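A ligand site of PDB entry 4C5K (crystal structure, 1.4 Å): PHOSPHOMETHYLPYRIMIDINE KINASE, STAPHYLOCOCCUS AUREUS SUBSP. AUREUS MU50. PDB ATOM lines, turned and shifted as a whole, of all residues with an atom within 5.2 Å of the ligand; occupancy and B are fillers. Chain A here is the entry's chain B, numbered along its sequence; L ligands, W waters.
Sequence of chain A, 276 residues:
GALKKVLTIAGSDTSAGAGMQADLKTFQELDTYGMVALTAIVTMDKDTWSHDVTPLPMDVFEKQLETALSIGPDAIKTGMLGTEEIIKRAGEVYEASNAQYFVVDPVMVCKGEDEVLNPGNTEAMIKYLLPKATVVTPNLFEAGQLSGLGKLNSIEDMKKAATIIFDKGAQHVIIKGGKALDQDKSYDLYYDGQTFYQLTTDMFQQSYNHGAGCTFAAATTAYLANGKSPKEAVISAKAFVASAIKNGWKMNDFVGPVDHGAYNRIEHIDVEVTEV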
ATOM      1  N   ASP A 105     -26.095  10.363 -14.521  1.00  0.00           N
ATOM      2  CA  ASP A 105     -27.032   9.970 -13.520  1.00  0.00           C
ATOM      3  C   ASP A 105     -28.336  10.659 -13.858  1.00  0.00           C
ATOM      4  O   ASP A 105     -28.432  11.874 -13.689  1.00  0.00           O
ATOM      5  CB  ASP A 105     -26.520  10.290 -12.134  1.00  0.00           C
ATOM      6  CG  ASP A 105     -27.313   9.624 -11.003  1.00  0.00           C
ATOM      7  OD1 ASP A 105     -27.989   8.603 -11.283  1.00  0.00           O
ATOM      8  OD2 ASP A 105     -27.215  10.058  -9.855  1.00  0.00           O
ATOM      9  N   ASN A 139     -32.193   4.810 -11.492  1.00  0.00           N
ATOM     10  CA  ASN A 139     -32.908   3.992 -10.550  1.00  0.00           C
ATOM     11  C   ASN A 139     -34.124   3.361 -11.268  1.00  0.00           C
ATOM     12  O   ASN A 139     -34.330   3.575 -12.488  1.00  0.00           O
ATOM     13  CB  ASN A 139     -33.295   4.719  -9.260  1.00  0.00           C
ATOM     14  CG  ASN A 139     -34.302   5.842  -9.479  1.00  0.00           C
ATOM     15  OD1 ASN A 139     -35.058   5.866 -10.461  1.00  0.00           O
ATOM     16  ND2 ASN A 139     -34.350   6.731  -8.555  1.00  0.00           N
ATOM     17  N   GLU A 142     -36.564   5.885 -12.901  1.00  0.00           N
ATOM     18  CA  GLU A 142     -35.920   6.552 -14.017  1.00  0.00           C
ATOM     19  C   GLU A 142     -35.764   5.649 -15.226  1.00  0.00           C
ATOM     20  O   GLU A 142     -35.916   6.089 -16.358  1.00  0.00           O
ATOM     21  CB  GLU A 142     -34.592   7.146 -13.605  1.00  0.00           C
ATOM     22  CG  GLU A 142     -34.714   8.248 -12.563  1.00  0.00           C
ATOM     23  CD  GLU A 142     -33.541   8.449 -11.610  1.00  0.00           C
ATOM     24  OE1 GLU A 142     -32.525   7.710 -11.763  1.00  0.00           O
ATOM     25  OE2 GLU A 142     -33.719   9.363 -10.756  1.00  0.00           O
ATOM     26  N   LYS A 176     -30.608   0.458 -11.123  1.00  0.00           N
ATOM     27  CA  LYS A 176     -30.632   0.150  -9.697  1.00  0.00           C
ATOM     28  C   LYS A 176     -32.031  -0.280  -9.270  1.00  0.00           C
ATOM     29  O   LYS A 176     -32.975   0.466  -9.462  1.00  0.00           O
ATOM     30  CB  LYS A 176     -30.156   1.339  -8.893  1.00  0.00           C
ATOM     31  CG  LYS A 176     -28.735   1.749  -9.235  1.00  0.00           C
ATOM     32  CD  LYS A 176     -28.375   3.146  -8.798  1.00  0.00           C
ATOM     33  CE  LYS A 176     -29.067   4.089  -9.728  1.00  0.00           C
ATOM     34  NZ  LYS A 176     -29.125   5.448  -9.193  1.00  0.00           N
ATOM     35  N   GLY A 177     -32.176  -1.445  -8.721  1.00  0.00           N
ATOM     36  CA  GLY A 177     -33.444  -1.880  -8.237  1.00  0.00           C
ATOM     37  C   GLY A 177     -33.644  -1.330  -6.855  1.00  0.00           C
ATOM     38  O   GLY A 177     -34.626  -0.674  -6.572  1.00  0.00           O
ATOM     39  N   GLY A 178     -32.747  -1.740  -5.974  1.00  0.00           N
ATOM     40  CA  GLY A 178     -32.777  -1.277  -4.589  1.00  0.00           C
ATOM     41  C   GLY A 178     -34.116  -1.539  -3.913  1.00  0.00           C
ATOM     42  O   GLY A 178     -34.800  -2.533  -4.233  1.00  0.00           O
ATOM     43  N   LYS A 179     -34.502  -0.634  -3.033  1.00  0.00           N
ATOM     44  CA  LYS A 179     -35.678  -0.799  -2.157  1.00  0.00           C
ATOM     45  C   LYS A 179     -36.948  -0.892  -3.000  1.00  0.00           C
ATOM     46  O   LYS A 179     -37.918  -1.522  -2.592  1.00  0.00           O
ATOM     47  CB  LYS A 179     -35.774   0.385  -1.152  1.00  0.00           C
ATOM     48  CG  LYS A 179     -34.415   0.744  -0.506  1.00  0.00           C
ATOM     49  CD  LYS A 179     -34.435   1.745   0.662  1.00  0.00           C
ATOM     50  CE  LYS A 179     -34.145   3.190   0.243  1.00  0.00           C
ATOM     51  NZ  LYS A 179     -32.812   3.431  -0.411  1.00  0.00           N
ATOM     52  N   SER A 186     -30.466  -6.197  -2.341  1.00  0.00           N
ATOM     53  CA  SER A 186     -30.370  -5.046  -3.202  1.00  0.00           C
ATOM     54  C   SER A 186     -29.827  -5.472  -4.568  1.00  0.00           C
ATOM     55  O   SER A 186     -28.601  -5.621  -4.747  1.00  0.00           O
ATOM     56  CB  SER A 186     -29.418  -4.016  -2.613  1.00  0.00           C
ATOM     57  OG  SER A 186     -29.450  -2.899  -3.432  1.00  0.00           O
ATOM     58  N   TYR A 187     -30.746  -5.594  -5.511  1.00  0.00           N
ATOM     59  CA  TYR A 187     -30.416  -6.036  -6.855  1.00  0.00           C
ATOM     60  C   TYR A 187     -30.319  -4.873  -7.798  1.00  0.00           C
ATOM     61  O   TYR A 187     -31.206  -4.019  -7.821  1.00  0.00           O
ATOM     62  CB  TYR A 187     -31.563  -6.871  -7.411  1.00  0.00           C
ATOM     63  CG  TYR A 187     -31.898  -8.147  -6.642  1.00  0.00           C
ATOM     64  CD1 TYR A 187     -31.190  -9.311  -6.885  1.00  0.00           C
ATOM     65  CD2 TYR A 187     -32.900  -8.205  -5.691  1.00  0.00           C
ATOM     66  CE1 TYR A 187     -31.432 -10.441  -6.257  1.00  0.00           C
ATOM     67  CE2 TYR A 187     -33.195  -9.401  -5.008  1.00  0.00           C
ATOM     68  CZ  TYR A 187     -32.446 -10.554  -5.263  1.00  0.00           C
ATOM     69  OH  TYR A 187     -32.707 -11.724  -4.607  1.00  0.00           O
ATOM     70  N   ASP A 188     -29.270  -4.876  -8.599  1.00  0.00           N
ATOM     71  CA  ASP A 188     -29.104  -4.014  -9.739  1.00  0.00           C
ATOM     72  C   ASP A 188     -28.877  -4.858 -10.991  1.00  0.00           C
ATOM     73  O   ASP A 188     -28.413  -5.986 -10.917  1.00  0.00           O
ATOM     74  CB  ASP A 188     -27.927  -3.037  -9.573  1.00  0.00           C
ATOM     75  CG  ASP A 188     -27.978  -2.221  -8.270  1.00  0.00           C
ATOM     76  OD1 ASP A 188     -29.086  -1.871  -7.786  1.00  0.00           O
ATOM     77  OD2 ASP A 188     -26.863  -1.987  -7.707  1.00  0.00           O
ATOM     78  N   THR A 201     -26.044  -7.243  -3.322  1.00  0.00           N
ATOM     79  CA  THR A 201     -25.552  -7.262  -1.950  1.00  0.00           C
ATOM     80  C   THR A 201     -26.746  -7.502  -1.034  1.00  0.00           C
ATOM     81  O   THR A 201     -27.901  -7.519  -1.494  1.00  0.00           O
ATOM     82  CB  THR A 201     -24.842  -5.967  -1.492  1.00  0.00           C
ATOM     83  OG1 THR A 201     -25.833  -4.941  -1.378  1.00  0.00           O
ATOM     84  CG2 THR A 201     -23.743  -5.545  -2.419  1.00  0.00           C
ATOM     85  N   ASP A 202     -26.473  -7.704   0.239  1.00  0.00           N
ATOM     86  CA  ASP A 202     -27.535  -7.709   1.221  1.00  0.00           C
ATOM     87  C   ASP A 202     -28.221  -6.315   1.146  1.00  0.00           C
ATOM     88  O   ASP A 202     -27.625  -5.311   0.719  1.00  0.00           O
ATOM     89  CB  ASP A 202     -27.039  -8.031   2.638  1.00  0.00           C
ATOM     90  CG  ASP A 202     -26.680  -9.511   2.823  1.00  0.00           C
ATOM     91  OD1 ASP A 202     -26.872 -10.351   1.901  1.00  0.00           O
ATOM     92  OD2 ASP A 202     -26.209  -9.828   3.931  1.00  0.00           O
ATOM     93  N   MET A 203     -29.480  -6.298   1.559  1.00  0.00           N
ATOM     94  CA  MET A 203     -30.203  -5.090   1.802  1.00  0.00           C
ATOM     95  C   MET A 203     -29.846  -4.675   3.228  1.00  0.00           C
ATOM     96  O   MET A 203     -30.011  -5.416   4.185  1.00  0.00           O
ATOM     97  CB  MET A 203     -31.719  -5.318   1.675  1.00  0.00           C
ATOM     98  CG  MET A 203     -32.583  -4.051   1.745  1.00  0.00           C
ATOM     99  SD  MET A 203     -32.263  -2.776   0.486  1.00  0.00           S
ATOM    100  CE  MET A 203     -33.059  -3.465  -0.945  1.00  0.00           C
ATOM    101  N   PHE A 204     -29.258  -3.506   3.350  1.00  0.00           N
ATOM    102  CA  PHE A 204     -28.890  -2.940   4.632  1.00  0.00           C
ATOM    103  C   PHE A 204     -29.972  -1.989   5.094  1.00  0.00           C
ATOM    104  O   PHE A 204     -30.989  -1.772   4.410  1.00  0.00           O
ATOM    105  CB  PHE A 204     -27.527  -2.224   4.482  1.00  0.00           C
ATOM    106  CG  PHE A 204     -26.406  -3.161   4.066  1.00  0.00           C
ATOM    107  CD1 PHE A 204     -25.983  -4.155   4.930  1.00  0.00           C
ATOM    108  CD2 PHE A 204     -25.862  -3.138   2.765  1.00  0.00           C
ATOM    109  CE1 PHE A 204     -25.008  -5.069   4.564  1.00  0.00           C
ATOM    110  CE2 PHE A 204     -24.864  -4.046   2.402  1.00  0.00           C
ATOM    111  CZ  PHE A 204     -24.436  -5.010   3.313  1.00  0.00           C
ATOM    112  N   GLN A 205     -29.731  -1.371   6.248  1.00  0.00           N
ATOM    113  CA  GLN A 205     -30.705  -0.445   6.790  1.00  0.00           C
ATOM    114  C   GLN A 205     -31.154   0.581   5.768  1.00  0.00           C
ATOM    115  O   GLN A 205     -30.367   1.067   4.974  1.00  0.00           O
ATOM    116  CB  GLN A 205     -30.194   0.212   8.060  1.00  0.00           C
ATOM    117  CG  GLN A 205     -28.986   1.136   7.931  1.00  0.00           C
ATOM    118  CD  GLN A 205     -29.344   2.512   7.400  1.00  0.00           C
ATOM    119  OE1 GLN A 205     -30.418   3.068   7.705  1.00  0.00           O
ATOM    120  NE2 GLN A 205     -28.400   3.120   6.683  1.00  0.00           N
ATOM    121  N   GLN A 206     -32.458   0.871   5.784  1.00  0.00           N
ATOM    122  CA  GLN A 206     -33.095   1.731   4.774  1.00  0.00           C
ATOM    123  C   GLN A 206     -33.438   3.118   5.286  1.00  0.00           C
ATOM    124  O   GLN A 206     -33.922   3.963   4.513  1.00  0.00           O
ATOM    125  CB  GLN A 206     -34.377   1.046   4.255  1.00  0.00           C
ATOM    126  CG  GLN A 206     -34.154  -0.357   3.706  1.00  0.00           C
ATOM    127  CD  GLN A 206     -35.426  -1.041   3.252  1.00  0.00           C
ATOM    128  OE1 GLN A 206     -36.539  -0.644   3.625  1.00  0.00           O
ATOM    129  NE2 GLN A 206     -35.280  -2.079   2.444  1.00  0.00           N
ATOM    130  N   ASN A 209     -30.175   6.630   3.985  1.00  0.00           N
ATOM    131  CA  ASN A 209     -29.652   6.306   2.658  1.00  0.00           C
ATOM    132  C   ASN A 209     -29.505   7.560   1.787  1.00  0.00           C
ATOM    133  O   ASN A 209     -29.384   7.474   0.586  1.00  0.00           O
ATOM    134  CB  ASN A 209     -30.565   5.318   1.914  1.00  0.00           C
ATOM    135  CG  ASN A 209     -30.691   3.943   2.583  1.00  0.00           C
ATOM    136  OD1 ASN A 209     -31.439   3.111   2.119  1.00  0.00           O
ATOM    137  ND2 ASN A 209     -29.974   3.712   3.672  1.00  0.00           N
ATOM    138  N   ALA A 212     -27.143   8.094  -1.591  1.00  0.00           N
ATOM    139  CA  ALA A 212     -26.703   6.828  -2.146  1.00  0.00           C
ATOM    140  C   ALA A 212     -26.574   6.858  -3.678  1.00  0.00           C
ATOM    141  O   ALA A 212     -25.612   6.371  -4.255  1.00  0.00           O
ATOM    142  CB  ALA A 212     -27.634   5.709  -1.681  1.00  0.00           C
ATOM    143  N   GLY A 213     -27.592   7.366  -4.358  1.00  0.00           N
ATOM    144  CA  GLY A 213     -27.551   7.389  -5.826  1.00  0.00           C
ATOM    145  C   GLY A 213     -26.448   8.270  -6.369  1.00  0.00           C
ATOM    146  O   GLY A 213     -25.700   7.861  -7.282  1.00  0.00           O
ATOM    147  N   PHE A 216     -23.159   6.511  -5.791  1.00  0.00           N
ATOM    148  CA  PHE A 216     -22.962   5.415  -6.752  1.00  0.00           C
ATOM    149  C   PHE A 216     -22.418   5.911  -8.094  1.00  0.00           C
ATOM    150  O   PHE A 216     -21.446   5.389  -8.651  1.00  0.00           O
ATOM    151  CB  PHE A 216     -24.254   4.627  -6.964  1.00  0.00           C
ATOM    152  CG  PHE A 216     -24.107   3.560  -8.004  1.00  0.00           C
ATOM    153  CD1 PHE A 216     -23.470   2.380  -7.715  1.00  0.00           C
ATOM    154  CD2 PHE A 216     -24.477   3.802  -9.292  1.00  0.00           C
ATOM    155  CE1 PHE A 216     -23.207   1.450  -8.693  1.00  0.00           C
ATOM    156  CE2 PHE A 216     -24.215   2.878 -10.283  1.00  0.00           C
ATOM    157  CZ  PHE A 216     -23.624   1.688  -9.973  1.00  0.00           C
ATOM    158  N   LYS A 238     -20.854  -0.242  -6.672  1.00  0.00           N
ATOM    159  CA  LYS A 238     -21.917  -0.839  -5.841  1.00  0.00           C
ATOM    160  C   LYS A 238     -21.358  -1.223  -4.475  1.00  0.00           C
ATOM    161  O   LYS A 238     -21.983  -1.003  -3.474  1.00  0.00           O
ATOM    162  CB  LYS A 238     -22.566  -2.051  -6.514  1.00  0.00           C
ATOM    163  CG  LYS A 238     -23.762  -2.587  -5.733  1.00  0.00           C
ATOM    164  CD  LYS A 238     -24.487  -3.691  -6.506  1.00  0.00           C
ATOM    165  CE  LYS A 238     -25.567  -4.325  -5.718  1.00  0.00           C
ATOM    166  NZ  LYS A 238     -26.621  -3.417  -5.224  1.00  0.00           N
ATOM    167  N   VAL A 241     -20.791   2.048  -2.421  1.00  0.00           N
ATOM    168  CA  VAL A 241     -21.974   2.632  -1.856  1.00  0.00           C
ATOM    169  C   VAL A 241     -22.662   1.708  -0.845  1.00  0.00           C
ATOM    170  O   VAL A 241     -23.287   2.189   0.104  1.00  0.00           O
ATOM    171  CB  VAL A 241     -22.911   3.149  -2.992  1.00  0.00           C
ATOM    172  CG1 VAL A 241     -23.661   2.006  -3.673  1.00  0.00           C
ATOM    173  CG2 VAL A 241     -23.850   4.215  -2.473  1.00  0.00           C
ATOM    174  N   ALA A 242     -22.521   0.384  -1.026  1.00  0.00           N
ATOM    175  CA  ALA A 242     -23.106  -0.518  -0.070  1.00  0.00           C
ATOM    176  C   ALA A 242     -22.510  -0.251   1.324  1.00  0.00           C
ATOM    177  O   ALA A 242     -23.204  -0.240   2.319  1.00  0.00           O
ATOM    178  CB  ALA A 242     -22.931  -1.952  -0.529  1.00  0.00           C
ATOM    179  N   ILE A 245     -23.901   2.976   2.697  1.00  0.00           N
ATOM    180  CA  ILE A 245     -25.278   2.794   3.144  1.00  0.00           C
ATOM    181  C   ILE A 245     -25.297   2.057   4.484  1.00  0.00           C
ATOM    182  O   ILE A 245     -25.960   2.463   5.449  1.00  0.00           O
ATOM    183  CB  ILE A 245     -26.101   2.032   2.077  1.00  0.00           C
ATOM    184  CG1 ILE A 245     -26.311   2.905   0.859  1.00  0.00           C
ATOM    185  CG2 ILE A 245     -27.423   1.503   2.616  1.00  0.00           C
ATOM    186  CD1 ILE A 245     -26.783   2.149  -0.345  1.00  0.00           C
HETATM  187  P1  LIG L   1     -31.381   6.400  -6.149  1.00  0.00           P
HETATM  188  O1  LIG L   1     -32.785   5.785  -6.008  1.00  0.00           O
HETATM  189  O2  LIG L   1     -30.941   7.184  -7.293  1.00  0.00           O
HETATM  190  O3  LIG L   1     -31.030   7.296  -4.969  1.00  0.00           O
HETATM  191  P2  LIG L   1     -30.695   3.965  -5.374  1.00  0.00           P
HETATM  192  O4  LIG L   1     -31.802   3.037  -6.111  1.00  0.00           O
HETATM  193  O5  LIG L   1     -30.739   4.640  -4.010  1.00  0.00           O
HETATM  194  O6  LIG L   1     -30.301   5.141  -6.288  1.00  0.00           O
HETATM  195  O7  LIG L   1     -29.415   3.014  -5.280  1.00  0.00           O
HETATM  196  C1  LIG L   1     -28.009   3.395  -5.194  1.00  0.00           C
HETATM  197  C2  LIG L   1     -27.247   2.095  -4.926  1.00  0.00           C
HETATM  198  O8  LIG L   1     -27.530   1.719  -3.583  1.00  0.00           O
HETATM  199  C3  LIG L   1     -27.630   0.897  -5.801  1.00  0.00           C
HETATM  200  O9  LIG L   1     -26.422   0.144  -6.105  1.00  0.00           O
HETATM  201  C4  LIG L   1     -28.664   0.165  -4.931  1.00  0.00           C
HETATM  202  O10 LIG L   1     -28.736  -1.229  -5.215  1.00  0.00           O
HETATM  203  C5  LIG L   1     -28.107   0.356  -3.545  1.00  0.00           C
HETATM  204  N1  LIG L   1     -28.984   0.418  -2.371  1.00  0.00           N
HETATM  205  C6  LIG L   1     -29.917   1.382  -2.124  1.00  0.00           C
HETATM  206  N2  LIG L   1     -30.473   1.209  -0.880  1.00  0.00           N
HETATM  207  C7  LIG L   1     -29.836   0.144  -0.327  1.00  0.00           C
HETATM  208  C8  LIG L   1     -29.949  -0.547   0.952  1.00  0.00           C
HETATM  209  N3  LIG L   1     -30.809  -0.097   1.876  1.00  0.00           N
HETATM  210  N4  LIG L   1     -29.145  -1.619   1.125  1.00  0.00           N
HETATM  211  C9  LIG L   1     -28.230  -2.022   0.209  1.00  0.00           C
HETATM  212  N5  LIG L   1     -28.072  -1.437  -1.001  1.00  0.00           N
HETATM  213  C10 LIG L   1     -28.861  -0.370  -1.306  1.00  0.00           C
HETATM  214  O   HOH W   1     -34.759   2.082  -7.499  1.00  0.00           O
HETATM  215  O   HOH W   2     -25.922  -2.655  -2.753  1.00  0.00           O
HETATM  216  O   HOH W   3     -30.396   7.795 -10.157  1.00  0.00           O
HETATM  217  O   HOH W   4     -35.096   6.889  -5.228  1.00  0.00           O
HETATM  218  O   HOH W   5     -32.331   9.602  -8.464  1.00  0.00           O
HETATM  219  O   HOH W   6     -29.035   9.486  -7.915  1.00  0.00           O
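The side-chain hydroxyl (OG) of Ser 186 is in hydrogen-bond range of an oxygen (O10) of the ligand, 2.5 Å away. An oxygen (O10) of the ligand is in hydrogen-bond range of the side-chain carboxylate of Asp 188, at 2.7 Å. The backbone NH of Phe 204 lies within hydrogen-bond range of a nitrogen (N4) of the ligand. A nitrogen (N3) of the ligand is in hydrogen-bond range of the backbone carbonyl oxygen of Phe 204 (3.0 Å). An oxygen (O10) of the ligand sits at hydrogen-bond distance from the side-chain amino group (NZ) of Lys 238 (3.0 Å). The side-chain amide nitrogen of Asn 139 lies within hydrogen-bond range of an oxygen (O1) of the ligand (3.1 Å). An oxygen (O2) of the ligand lies within salt-bridge range of the side-chain amino group (NZ) of Lys 176, 3.1 Å away. SD of Met 203 lies close to N3 of the ligand, 3.4 Å away. NZ of Lys 179 sits at hydrogen-bond distance from N2 of the ligand (3.3 Å). The side-chain amide oxygen of Asn 209 is in hydrogen-bond range of a nitrogen (N3) of the ligand (3.3 Å). O of Gln 205 is in hydrogen-bond range of N3 of the ligand (3.3 Å). O3 of the ligand lies within hydrogen-bond range of N of Gly 213.
Merely in contact with the ligand: Ile 245 (3.4 Å), Asp 202 (3.4 Å), Val 241 (3.8 Å), Gln 206 (3.8 Å) and Ala 212 (3.9 Å). Within 4 Å of the ligand: Asn 139, Lys 176, Lys 179, Ser 186, Asp 188, Asp 202, Met 203, Phe 204, Gln 205, Gln 206, Asn 209, Ala 212, Gly 213, Lys 238, Val 241 and Ile 245.
NZ of Lys 238 lies within hydrogen-bond range of O of Ser 186, at 3.0 Å. The backbone NH of Ser 186 sits at hydrogen-bond distance from the backbone carbonyl oxygen of Thr 201 (3.0 Å). The side-chain amino group of Lys 238 is in salt-bridge range of the side-chain carboxylate of Asp 188, at 2.9 Å. The side-chain carboxylate of Asp 188 lies within hydrogen-bond range of the backbone NH of Gly 177 (3.3 Å). The backbone NH (N) of Glu 142 sits at hydrogen-bond distance from the side-chain amide oxygen (OD1) of Asn 139, at 2.9 Å. The side-chain amino group (NZ) of Lys 176 is in salt-bridge range of the side-chain carboxylate (OD1) of Asp 105. The side-chain amide nitrogen of Gln 206 sits close to the side-chain sulfur of Met 203 (3.7 Å). The side-chain amide nitrogen (ND2) of Asn 209 sits at hydrogen-bond distance from the backbone carbonyl oxygen (O) of Gln 205 (3.0 Å).
Water W4 lies within hydrogen-bond range of an oxygen (O1) of the ligand (2.7 Å) and the side-chain amide nitrogen of Asn 139 (3.4 Å). Water W3 lies within hydrogen-bond range of the side-chain carboxylate of Glu 142 (2.7 Å), the side-chain carboxylate of Asp 105 (2.8 Å), the side-chain amino group of Lys 176 (2.8 Å) and an oxygen (O2) of the ligand (3.0 Å). Water W5 lies within hydrogen-bond range of OE2 of Glu 142 (2.7 Å) and O2 of the ligand (3.0 Å). Water W2 lies within hydrogen-bond range of OG1 of Thr 201 (2.7 Å), NZ of Lys 238 (2.7 Å) and N5 of the ligand (3.0 Å). Water W6 bridges OD2 of Asp 105 (2.7 Å) and O2 of the ligand (3.1 Å). Water W1 lies within hydrogen-bond range of the backbone carbonyl oxygen (O) of Gly 177 (2.9 Å), the backbone carbonyl oxygen (O) of Lys 176 (3.1 Å) and an oxygen (O4) of the ligand (3.4 Å).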
